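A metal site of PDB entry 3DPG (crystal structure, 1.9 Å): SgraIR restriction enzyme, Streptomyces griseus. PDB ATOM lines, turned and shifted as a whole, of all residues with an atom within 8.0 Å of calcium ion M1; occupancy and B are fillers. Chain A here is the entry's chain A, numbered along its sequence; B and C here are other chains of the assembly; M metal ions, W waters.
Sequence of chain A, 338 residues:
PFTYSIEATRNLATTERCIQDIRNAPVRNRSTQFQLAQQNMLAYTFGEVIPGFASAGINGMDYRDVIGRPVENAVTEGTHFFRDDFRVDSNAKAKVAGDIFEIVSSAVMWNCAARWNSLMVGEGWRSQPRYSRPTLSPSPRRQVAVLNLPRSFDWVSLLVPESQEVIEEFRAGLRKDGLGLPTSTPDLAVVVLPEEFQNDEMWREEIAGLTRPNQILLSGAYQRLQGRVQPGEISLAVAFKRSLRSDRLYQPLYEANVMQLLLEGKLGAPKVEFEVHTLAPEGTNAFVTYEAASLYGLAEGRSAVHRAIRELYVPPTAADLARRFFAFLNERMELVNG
The side-chain hydroxyl (OG) of Ser 106 lies within hydrogen-bond range of the backbone carbonyl oxygen (O) of Glu 102 (2.9 Å).
The backbone NH of Leu 149 lies within hydrogen-bond range of the backbone carbonyl oxygen of Asp 187 (2.9 Å).
Along chain A the residues within 4 Å of calcium ion M1 span positions 102 to 149.
O of Leu 149 binds calcium ion M1 (2.5 Å).
OD1 of Asn 148 binds calcium ion M1, at 2.5 Å.
Calcium ion M1 is bound by OE2 of Glu 102, at 2.5 Å.
Water W2 binds calcium ion M1 (2.6 Å).
Calcium ion M1 is bound by water W3 (2.8 Å).
Slightly farther from calcium ion M1 lies water W1 (3.0 Å).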
ATOM      1  N   ASP A  99     -19.310 -13.601  -4.664  1.00  0.00           N
ATOM      2  CA  ASP A  99     -20.182 -12.489  -5.007  1.00  0.00           C
ATOM      3  C   ASP A  99     -21.245 -12.227  -3.942  1.00  0.00           C
ATOM      4  O   ASP A  99     -21.539 -11.073  -3.648  1.00  0.00           O
ATOM      5  CB  ASP A  99     -20.817 -12.675  -6.394  1.00  0.00           C
ATOM      6  CG  ASP A  99     -19.883 -12.278  -7.525  1.00  0.00           C
ATOM      7  OD1 ASP A  99     -18.706 -11.957  -7.244  1.00  0.00           O
ATOM      8  OD2 ASP A  99     -20.314 -12.285  -8.691  1.00  0.00           O
ATOM      9  N   GLU A 102     -19.519 -10.308  -1.078  1.00  0.00           N
ATOM     10  CA  GLU A 102     -19.299  -8.909  -1.412  1.00  0.00           C
ATOM     11  C   GLU A 102     -20.591  -8.105  -1.502  1.00  0.00           C
ATOM     12  O   GLU A 102     -20.722  -7.046  -0.892  1.00  0.00           O
ATOM     13  CB  GLU A 102     -18.508  -8.780  -2.709  1.00  0.00           C
ATOM     14  CG  GLU A 102     -18.476  -7.355  -3.202  1.00  0.00           C
ATOM     15  CD  GLU A 102     -17.692  -7.199  -4.462  1.00  0.00           C
ATOM     16  OE1 GLU A 102     -17.216  -8.211  -5.010  1.00  0.00           O
ATOM     17  OE2 GLU A 102     -17.547  -6.041  -4.891  1.00  0.00           O
ATOM     18  N   ILE A 103     -21.576  -8.613  -2.243  1.00  0.00           N
ATOM     19  CA  ILE A 103     -22.805  -7.864  -2.478  1.00  0.00           C
ATOM     20  C   ILE A 103     -23.591  -7.634  -1.195  1.00  0.00           C
ATOM     21  O   ILE A 103     -23.997  -6.510  -0.891  1.00  0.00           O
ATOM     22  CB  ILE A 103     -23.670  -8.543  -3.548  1.00  0.00           C
ATOM     23  CG1 ILE A 103     -22.962  -8.486  -4.908  1.00  0.00           C
ATOM     24  CG2 ILE A 103     -25.016  -7.853  -3.648  1.00  0.00           C
ATOM     25  CD1 ILE A 103     -23.514  -9.473  -5.936  1.00  0.00           C
ATOM     26  N   SER A 106     -21.777  -5.191   1.091  1.00  0.00           N
ATOM     27  CA  SER A 106     -21.929  -3.853   0.537  1.00  0.00           C
ATOM     28  C   SER A 106     -23.308  -3.275   0.805  1.00  0.00           C
ATOM     29  O   SER A 106     -23.441  -2.072   1.003  1.00  0.00           O
ATOM     30  CB  SER A 106     -21.640  -3.876  -0.958  1.00  0.00           C
ATOM     31  OG  SER A 106     -20.293  -4.216  -1.179  1.00  0.00           O
ATOM     32  N   LEU A 147     -20.039   2.732  -2.590  1.00  0.00           N
ATOM     33  CA  LEU A 147     -19.988   2.350  -4.001  1.00  0.00           C
ATOM     34  C   LEU A 147     -19.420   0.959  -4.233  1.00  0.00           C
ATOM     35  O   LEU A 147     -18.209   0.744  -4.176  1.00  0.00           O
ATOM     36  CB  LEU A 147     -19.137   3.353  -4.794  1.00  0.00           C
ATOM     37  CG  LEU A 147     -19.438   4.850  -4.630  1.00  0.00           C
ATOM     38  CD1 LEU A 147     -18.392   5.678  -5.390  1.00  0.00           C
ATOM     39  CD2 LEU A 147     -20.856   5.172  -5.111  1.00  0.00           C
ATOM     40  N   ASN A 148     -20.304   0.025  -4.512  1.00  0.00           N
ATOM     41  CA  ASN A 148     -19.879  -1.281  -4.981  1.00  0.00           C
ATOM     42  C   ASN A 148     -19.313  -1.108  -6.395  1.00  0.00           C
ATOM     43  O   ASN A 148     -20.043  -0.739  -7.314  1.00  0.00           O
ATOM     44  CB  ASN A 148     -21.059  -2.264  -4.953  1.00  0.00           C
ATOM     45  CG  ASN A 148     -20.640  -3.649  -5.330  1.00  0.00           C
ATOM     46  OD1 ASN A 148     -19.555  -3.823  -5.852  1.00  0.00           O
ATOM     47  ND2 ASN A 148     -21.483  -4.645  -5.069  1.00  0.00           N
ATOM     48  N   LEU A 149     -18.021  -1.352  -6.568  1.00  0.00           N
ATOM     49  CA  LEU A 149     -17.381  -1.093  -7.864  1.00  0.00           C
ATOM     50  C   LEU A 149     -17.431  -2.329  -8.758  1.00  0.00           C
ATOM     51  O   LEU A 149     -17.300  -3.445  -8.269  1.00  0.00           O
ATOM     52  CB  LEU A 149     -15.929  -0.606  -7.672  1.00  0.00           C
ATOM     53  CG  LEU A 149     -15.845   0.580  -6.708  1.00  0.00           C
ATOM     54  CD1 LEU A 149     -14.396   1.020  -6.468  1.00  0.00           C
ATOM     55  CD2 LEU A 149     -16.688   1.756  -7.225  1.00  0.00           C
ATOM     56  N   PRO A 150     -17.616  -2.128 -10.066  1.00  0.00           N
ATOM     57  CA  PRO A 150     -17.781  -3.251 -11.000  1.00  0.00           C
ATOM     58  C   PRO A 150     -16.474  -3.901 -11.425  1.00  0.00           C
ATOM     59  O   PRO A 150     -15.416  -3.303 -11.314  1.00  0.00           O
ATOM     60  CB  PRO A 150     -18.417  -2.598 -12.231  1.00  0.00           C
ATOM     61  CG  PRO A 150     -17.960  -1.190 -12.180  1.00  0.00           C
ATOM     62  CD  PRO A 150     -17.790  -0.828 -10.732  1.00  0.00           C
ATOM     63  N   ARG A 151     -16.571  -5.122 -11.947  1.00  0.00           N
ATOM     64  CA  ARG A 151     -15.411  -5.787 -12.527  1.00  0.00           C
ATOM     65  C   ARG A 151     -14.891  -4.903 -13.658  1.00  0.00           C
ATOM     66  O   ARG A 151     -15.669  -4.291 -14.387  1.00  0.00           O
ATOM     67  CB  ARG A 151     -15.805  -7.178 -13.044  1.00  0.00           C
ATOM     68  CG  ARG A 151     -16.111  -8.195 -11.947  1.00  0.00           C
ATOM     69  CD  ARG A 151     -16.619  -9.526 -12.528  1.00  0.00           C
ATOM     70  NE  ARG A 151     -16.270 -10.677 -11.690  1.00  0.00           N
ATOM     71  CZ  ARG A 151     -17.021 -11.143 -10.702  1.00  0.00           C
ATOM     72  NH1 ARG A 151     -18.183 -10.562 -10.419  1.00  0.00           N
ATOM     73  NH2 ARG A 151     -16.617 -12.196  -9.997  1.00  0.00           N
ATOM     74  N   PHE A 153     -13.291  -2.128 -13.374  1.00  0.00           N
ATOM     75  CA  PHE A 153     -13.327  -0.715 -13.011  1.00  0.00           C
ATOM     76  C   PHE A 153     -11.918  -0.166 -12.790  1.00  0.00           C
ATOM     77  O   PHE A 153     -11.021  -0.877 -12.334  1.00  0.00           O
ATOM     78  CB  PHE A 153     -14.159  -0.523 -11.741  1.00  0.00           C
ATOM     79  CG  PHE A 153     -14.478   0.912 -11.440  1.00  0.00           C
ATOM     80  CD1 PHE A 153     -15.287   1.656 -12.295  1.00  0.00           C
ATOM     81  CD2 PHE A 153     -14.013   1.517 -10.282  1.00  0.00           C
ATOM     82  CE1 PHE A 153     -15.607   2.971 -12.002  1.00  0.00           C
ATOM     83  CE2 PHE A 153     -14.323   2.834 -10.002  1.00  0.00           C
ATOM     84  CZ  PHE A 153     -15.119   3.559 -10.858  1.00  0.00           C
ATOM     85  N   THR A 185      -8.880  -1.845  -9.102  1.00  0.00           N
ATOM     86  CA  THR A 185      -9.947  -1.332  -8.255  1.00  0.00           C
ATOM     87  C   THR A 185     -10.103  -2.179  -7.003  1.00  0.00           C
ATOM     88  O   THR A 185      -9.925  -3.396  -7.050  1.00  0.00           O
ATOM     89  CB  THR A 185     -11.291  -1.343  -9.018  1.00  0.00           C
ATOM     90  OG1 THR A 185     -12.321  -0.760  -8.195  1.00  0.00           O
ATOM     91  CG2 THR A 185     -11.686  -2.767  -9.379  1.00  0.00           C
ATOM     92  N   PRO A 186     -10.466  -1.541  -5.872  1.00  0.00           N
ATOM     93  CA  PRO A 186     -10.936  -2.340  -4.753  1.00  0.00           C
ATOM     94  C   PRO A 186     -12.350  -2.811  -5.097  1.00  0.00           C
ATOM     95  O   PRO A 186     -12.896  -2.322  -6.088  1.00  0.00           O
ATOM     96  CB  PRO A 186     -11.029  -1.338  -3.612  1.00  0.00           C
ATOM     97  CG  PRO A 186     -10.682   0.021  -4.196  1.00  0.00           C
ATOM     98  CD  PRO A 186     -10.723  -0.107  -5.670  1.00  0.00           C
ATOM     99  N   ASP A 187     -12.909  -3.726  -4.320  1.00  0.00           N
ATOM    100  CA  ASP A 187     -14.300  -4.143  -4.534  1.00  0.00           C
ATOM    101  C   ASP A 187     -15.238  -2.990  -4.271  1.00  0.00           C
ATOM    102  O   ASP A 187     -16.285  -2.885  -4.892  1.00  0.00           O
ATOM    103  CB  ASP A 187     -14.687  -5.218  -3.540  1.00  0.00           C
ATOM    104  CG  ASP A 187     -14.027  -6.530  -3.834  1.00  0.00           C
ATOM    105  OD1 ASP A 187     -13.877  -6.863  -5.025  1.00  0.00           O
ATOM    106  OD2 ASP A 187     -13.669  -7.221  -2.863  1.00  0.00           O
ATOM    107  N   LEU A 188     -14.865  -2.148  -3.320  1.00  0.00           N
ATOM    108  CA  LEU A 188     -15.800  -1.125  -2.855  1.00  0.00           C
ATOM    109  C   LEU A 188     -15.082   0.117  -2.378  1.00  0.00           C
ATOM    110  O   LEU A 188     -13.997   0.045  -1.810  1.00  0.00           O
ATOM    111  CB  LEU A 188     -16.693  -1.701  -1.747  1.00  0.00           C
ATOM    112  CG  LEU A 188     -17.733  -0.808  -1.091  1.00  0.00           C
ATOM    113  CD1 LEU A 188     -18.928  -1.647  -0.642  1.00  0.00           C
ATOM    114  CD2 LEU A 188     -17.123  -0.026   0.079  1.00  0.00           C
ATOM    115  N   SER A 219     -25.513  -1.532  -7.185  1.00  0.00           N
ATOM    116  CA  SER A 219     -24.422  -1.835  -8.095  1.00  0.00           C
ATOM    117  C   SER A 219     -24.173  -0.719  -9.108  1.00  0.00           C
ATOM    118  O   SER A 219     -23.059  -0.567  -9.608  1.00  0.00           O
ATOM    119  CB  SER A 219     -24.633  -3.190  -8.788  1.00  0.00           C
ATOM    120  OG  SER A 219     -25.638  -3.092  -9.777  1.00  0.00           O
ATOM    121  N   PHE A 240     -13.155  -7.584  -0.411  1.00  0.00           N
ATOM    122  CA  PHE A 240     -13.815  -8.737   0.201  1.00  0.00           C
ATOM    123  C   PHE A 240     -13.222 -10.022  -0.333  1.00  0.00           C
ATOM    124  O   PHE A 240     -13.075 -10.193  -1.543  1.00  0.00           O
ATOM    125  CB  PHE A 240     -15.317  -8.715  -0.103  1.00  0.00           C
ATOM    126  CG  PHE A 240     -16.033  -7.516   0.431  1.00  0.00           C
ATOM    127  CD1 PHE A 240     -16.397  -7.436   1.758  1.00  0.00           C
ATOM    128  CD2 PHE A 240     -16.345  -6.470  -0.419  1.00  0.00           C
ATOM    129  CE1 PHE A 240     -17.056  -6.336   2.252  1.00  0.00           C
ATOM    130  CE2 PHE A 240     -17.017  -5.353   0.076  1.00  0.00           C
ATOM    131  CZ  PHE A 240     -17.365  -5.295   1.411  1.00  0.00           C
ATOM    132  P    DA B   7     -11.018  -7.120 -13.119  1.00  0.00           P
ATOM    133  OP1  DA B   7     -11.447  -5.843 -12.503  1.00  0.00           O
ATOM    134  OP2  DA B   7      -9.596  -7.320 -13.495  1.00  0.00           O
ATOM    135  O5'  DA B   7     -11.443  -8.313 -12.155  1.00  0.00           O
ATOM    136  C5'  DA B   7     -12.672  -8.180 -11.493  1.00  0.00           C
ATOM    137  C4'  DA B   7     -12.987  -9.462 -10.760  1.00  0.00           C
ATOM    138  O4'  DA B   7     -13.062 -10.539 -11.713  1.00  0.00           O
ATOM    139  C3'  DA B   7     -11.960  -9.890  -9.731  1.00  0.00           C
ATOM    140  O3'  DA B   7     -12.726  -9.932  -8.561  1.00  0.00           O
ATOM    141  C2'  DA B   7     -11.519 -11.290 -10.167  1.00  0.00           C
ATOM    142  C1'  DA B   7     -12.682 -11.715 -11.055  1.00  0.00           C
ATOM    143  N9   DA B   7     -12.354 -12.654 -12.126  1.00  0.00           N
ATOM    144  C8   DA B   7     -11.272 -12.611 -12.960  1.00  0.00           C
ATOM    145  N7   DA B   7     -11.237 -13.585 -13.844  1.00  0.00           N
ATOM    146  C5   DA B   7     -12.381 -14.306 -13.564  1.00  0.00           C
ATOM    147  C6   DA B   7     -12.921 -15.469 -14.162  1.00  0.00           C
ATOM    148  N6   DA B   7     -12.329 -16.105 -15.181  1.00  0.00           N
ATOM    149  N1   DA B   7     -14.070 -15.939 -13.656  1.00  0.00           N
ATOM    150  C2   DA B   7     -14.646 -15.292 -12.638  1.00  0.00           C
ATOM    151  N3   DA B   7     -14.240 -14.198 -11.994  1.00  0.00           N
ATOM    152  C4   DA B   7     -13.085 -13.755 -12.515  1.00  0.00           C
ATOM    153  P    DC B   8     -12.191 -10.390  -7.145  1.00  0.00           P
ATOM    154  OP1  DC B   8     -12.737  -9.402  -6.212  1.00  0.00           O
ATOM    155  OP2  DC B   8     -10.724 -10.657  -7.201  1.00  0.00           O
ATOM    156  O5'  DC B   8     -12.975 -11.767  -6.936  1.00  0.00           O
ATOM    157  C5'  DC B   8     -14.380 -11.712  -6.618  1.00  0.00           C
ATOM    158  C4'  DC B   8     -14.959 -13.119  -6.609  1.00  0.00           C
ATOM    159  O4'  DC B   8     -14.893 -13.680  -7.944  1.00  0.00           O
ATOM    160  C3'  DC B   8     -14.188 -14.123  -5.756  1.00  0.00           C
ATOM    161  O3'  DC B   8     -14.680 -14.034  -4.453  1.00  0.00           O
ATOM    162  C2'  DC B   8     -14.555 -15.464  -6.406  1.00  0.00           C
ATOM    163  C1'  DC B   8     -14.708 -15.081  -7.871  1.00  0.00           C
ATOM    164  N1   DC B   8     -13.532 -15.436  -8.739  1.00  0.00           N
ATOM    165  C2   DC B   8     -13.506 -16.694  -9.348  1.00  0.00           C
ATOM    166  O2   DC B   8     -14.421 -17.481  -9.144  1.00  0.00           O
ATOM    167  N3   DC B   8     -12.449 -17.019 -10.133  1.00  0.00           N
ATOM    168  C4   DC B   8     -11.470 -16.149 -10.331  1.00  0.00           C
ATOM    169  N4   DC B   8     -10.468 -16.534 -11.126  1.00  0.00           N
ATOM    170  C5   DC B   8     -11.473 -14.853  -9.712  1.00  0.00           C
ATOM    171  C6   DC B   8     -12.521 -14.543  -8.937  1.00  0.00           C
ATOM    172  P    DA C  15     -24.937  -8.435 -13.557  1.00  0.00           P
ATOM    173  OP1  DA C  15     -24.987  -8.403 -12.074  1.00  0.00           O
ATOM    174  OP2  DA C  15     -26.199  -8.474 -14.335  1.00  0.00           O
ATOM    175  O5'  DA C  15     -24.062  -7.205 -14.098  1.00  0.00           O
ATOM    176  C5'  DA C  15     -22.755  -6.966 -13.597  1.00  0.00           C
ATOM    177  C4'  DA C  15     -21.954  -6.047 -14.503  1.00  0.00           C
ATOM    178  O4'  DA C  15     -21.297  -6.828 -15.526  1.00  0.00           O
ATOM    179  C3'  DA C  15     -22.750  -4.956 -15.219  1.00  0.00           C
ATOM    180  O3'  DA C  15     -22.075  -3.687 -15.125  1.00  0.00           O
ATOM    181  C2'  DA C  15     -22.861  -5.456 -16.666  1.00  0.00           C
ATOM    182  C1'  DA C  15     -21.790  -6.537 -16.813  1.00  0.00           C
ATOM    183  N9   DA C  15     -22.271  -7.802 -17.361  1.00  0.00           N
ATOM    184  C8   DA C  15     -23.447  -8.425 -17.073  1.00  0.00           C
ATOM    185  N7   DA C  15     -23.610  -9.569 -17.699  1.00  0.00           N
ATOM    186  C5   DA C  15     -22.460  -9.711 -18.454  1.00  0.00           C
ATOM    187  C6   DA C  15     -22.019 -10.708 -19.336  1.00  0.00           C
ATOM    188  N6   DA C  15     -22.731 -11.801 -19.613  1.00  0.00           N
ATOM    189  N1   DA C  15     -20.819 -10.538 -19.922  1.00  0.00           N
ATOM    190  C2   DA C  15     -20.107  -9.445 -19.646  1.00  0.00           C
ATOM    191  N3   DA C  15     -20.418  -8.442 -18.824  1.00  0.00           N
ATOM    192  C4   DA C  15     -21.618  -8.629 -18.256  1.00  0.00           C
HETATM  193 CA    CA M   1     -18.301  -5.510  -7.264  1.00  0.00          CA
HETATM  194 CA    CA M   2     -12.957  -9.340  -3.859  1.00  0.00          CA
HETATM  195  O   HOH W   1     -15.366  -5.732  -7.556  1.00  0.00           O
HETATM  196  O   HOH W   2     -18.070  -7.547  -8.939  1.00  0.00           O
HETATM  197  O   HOH W   3     -20.619  -7.100  -7.100  1.00  0.00           O
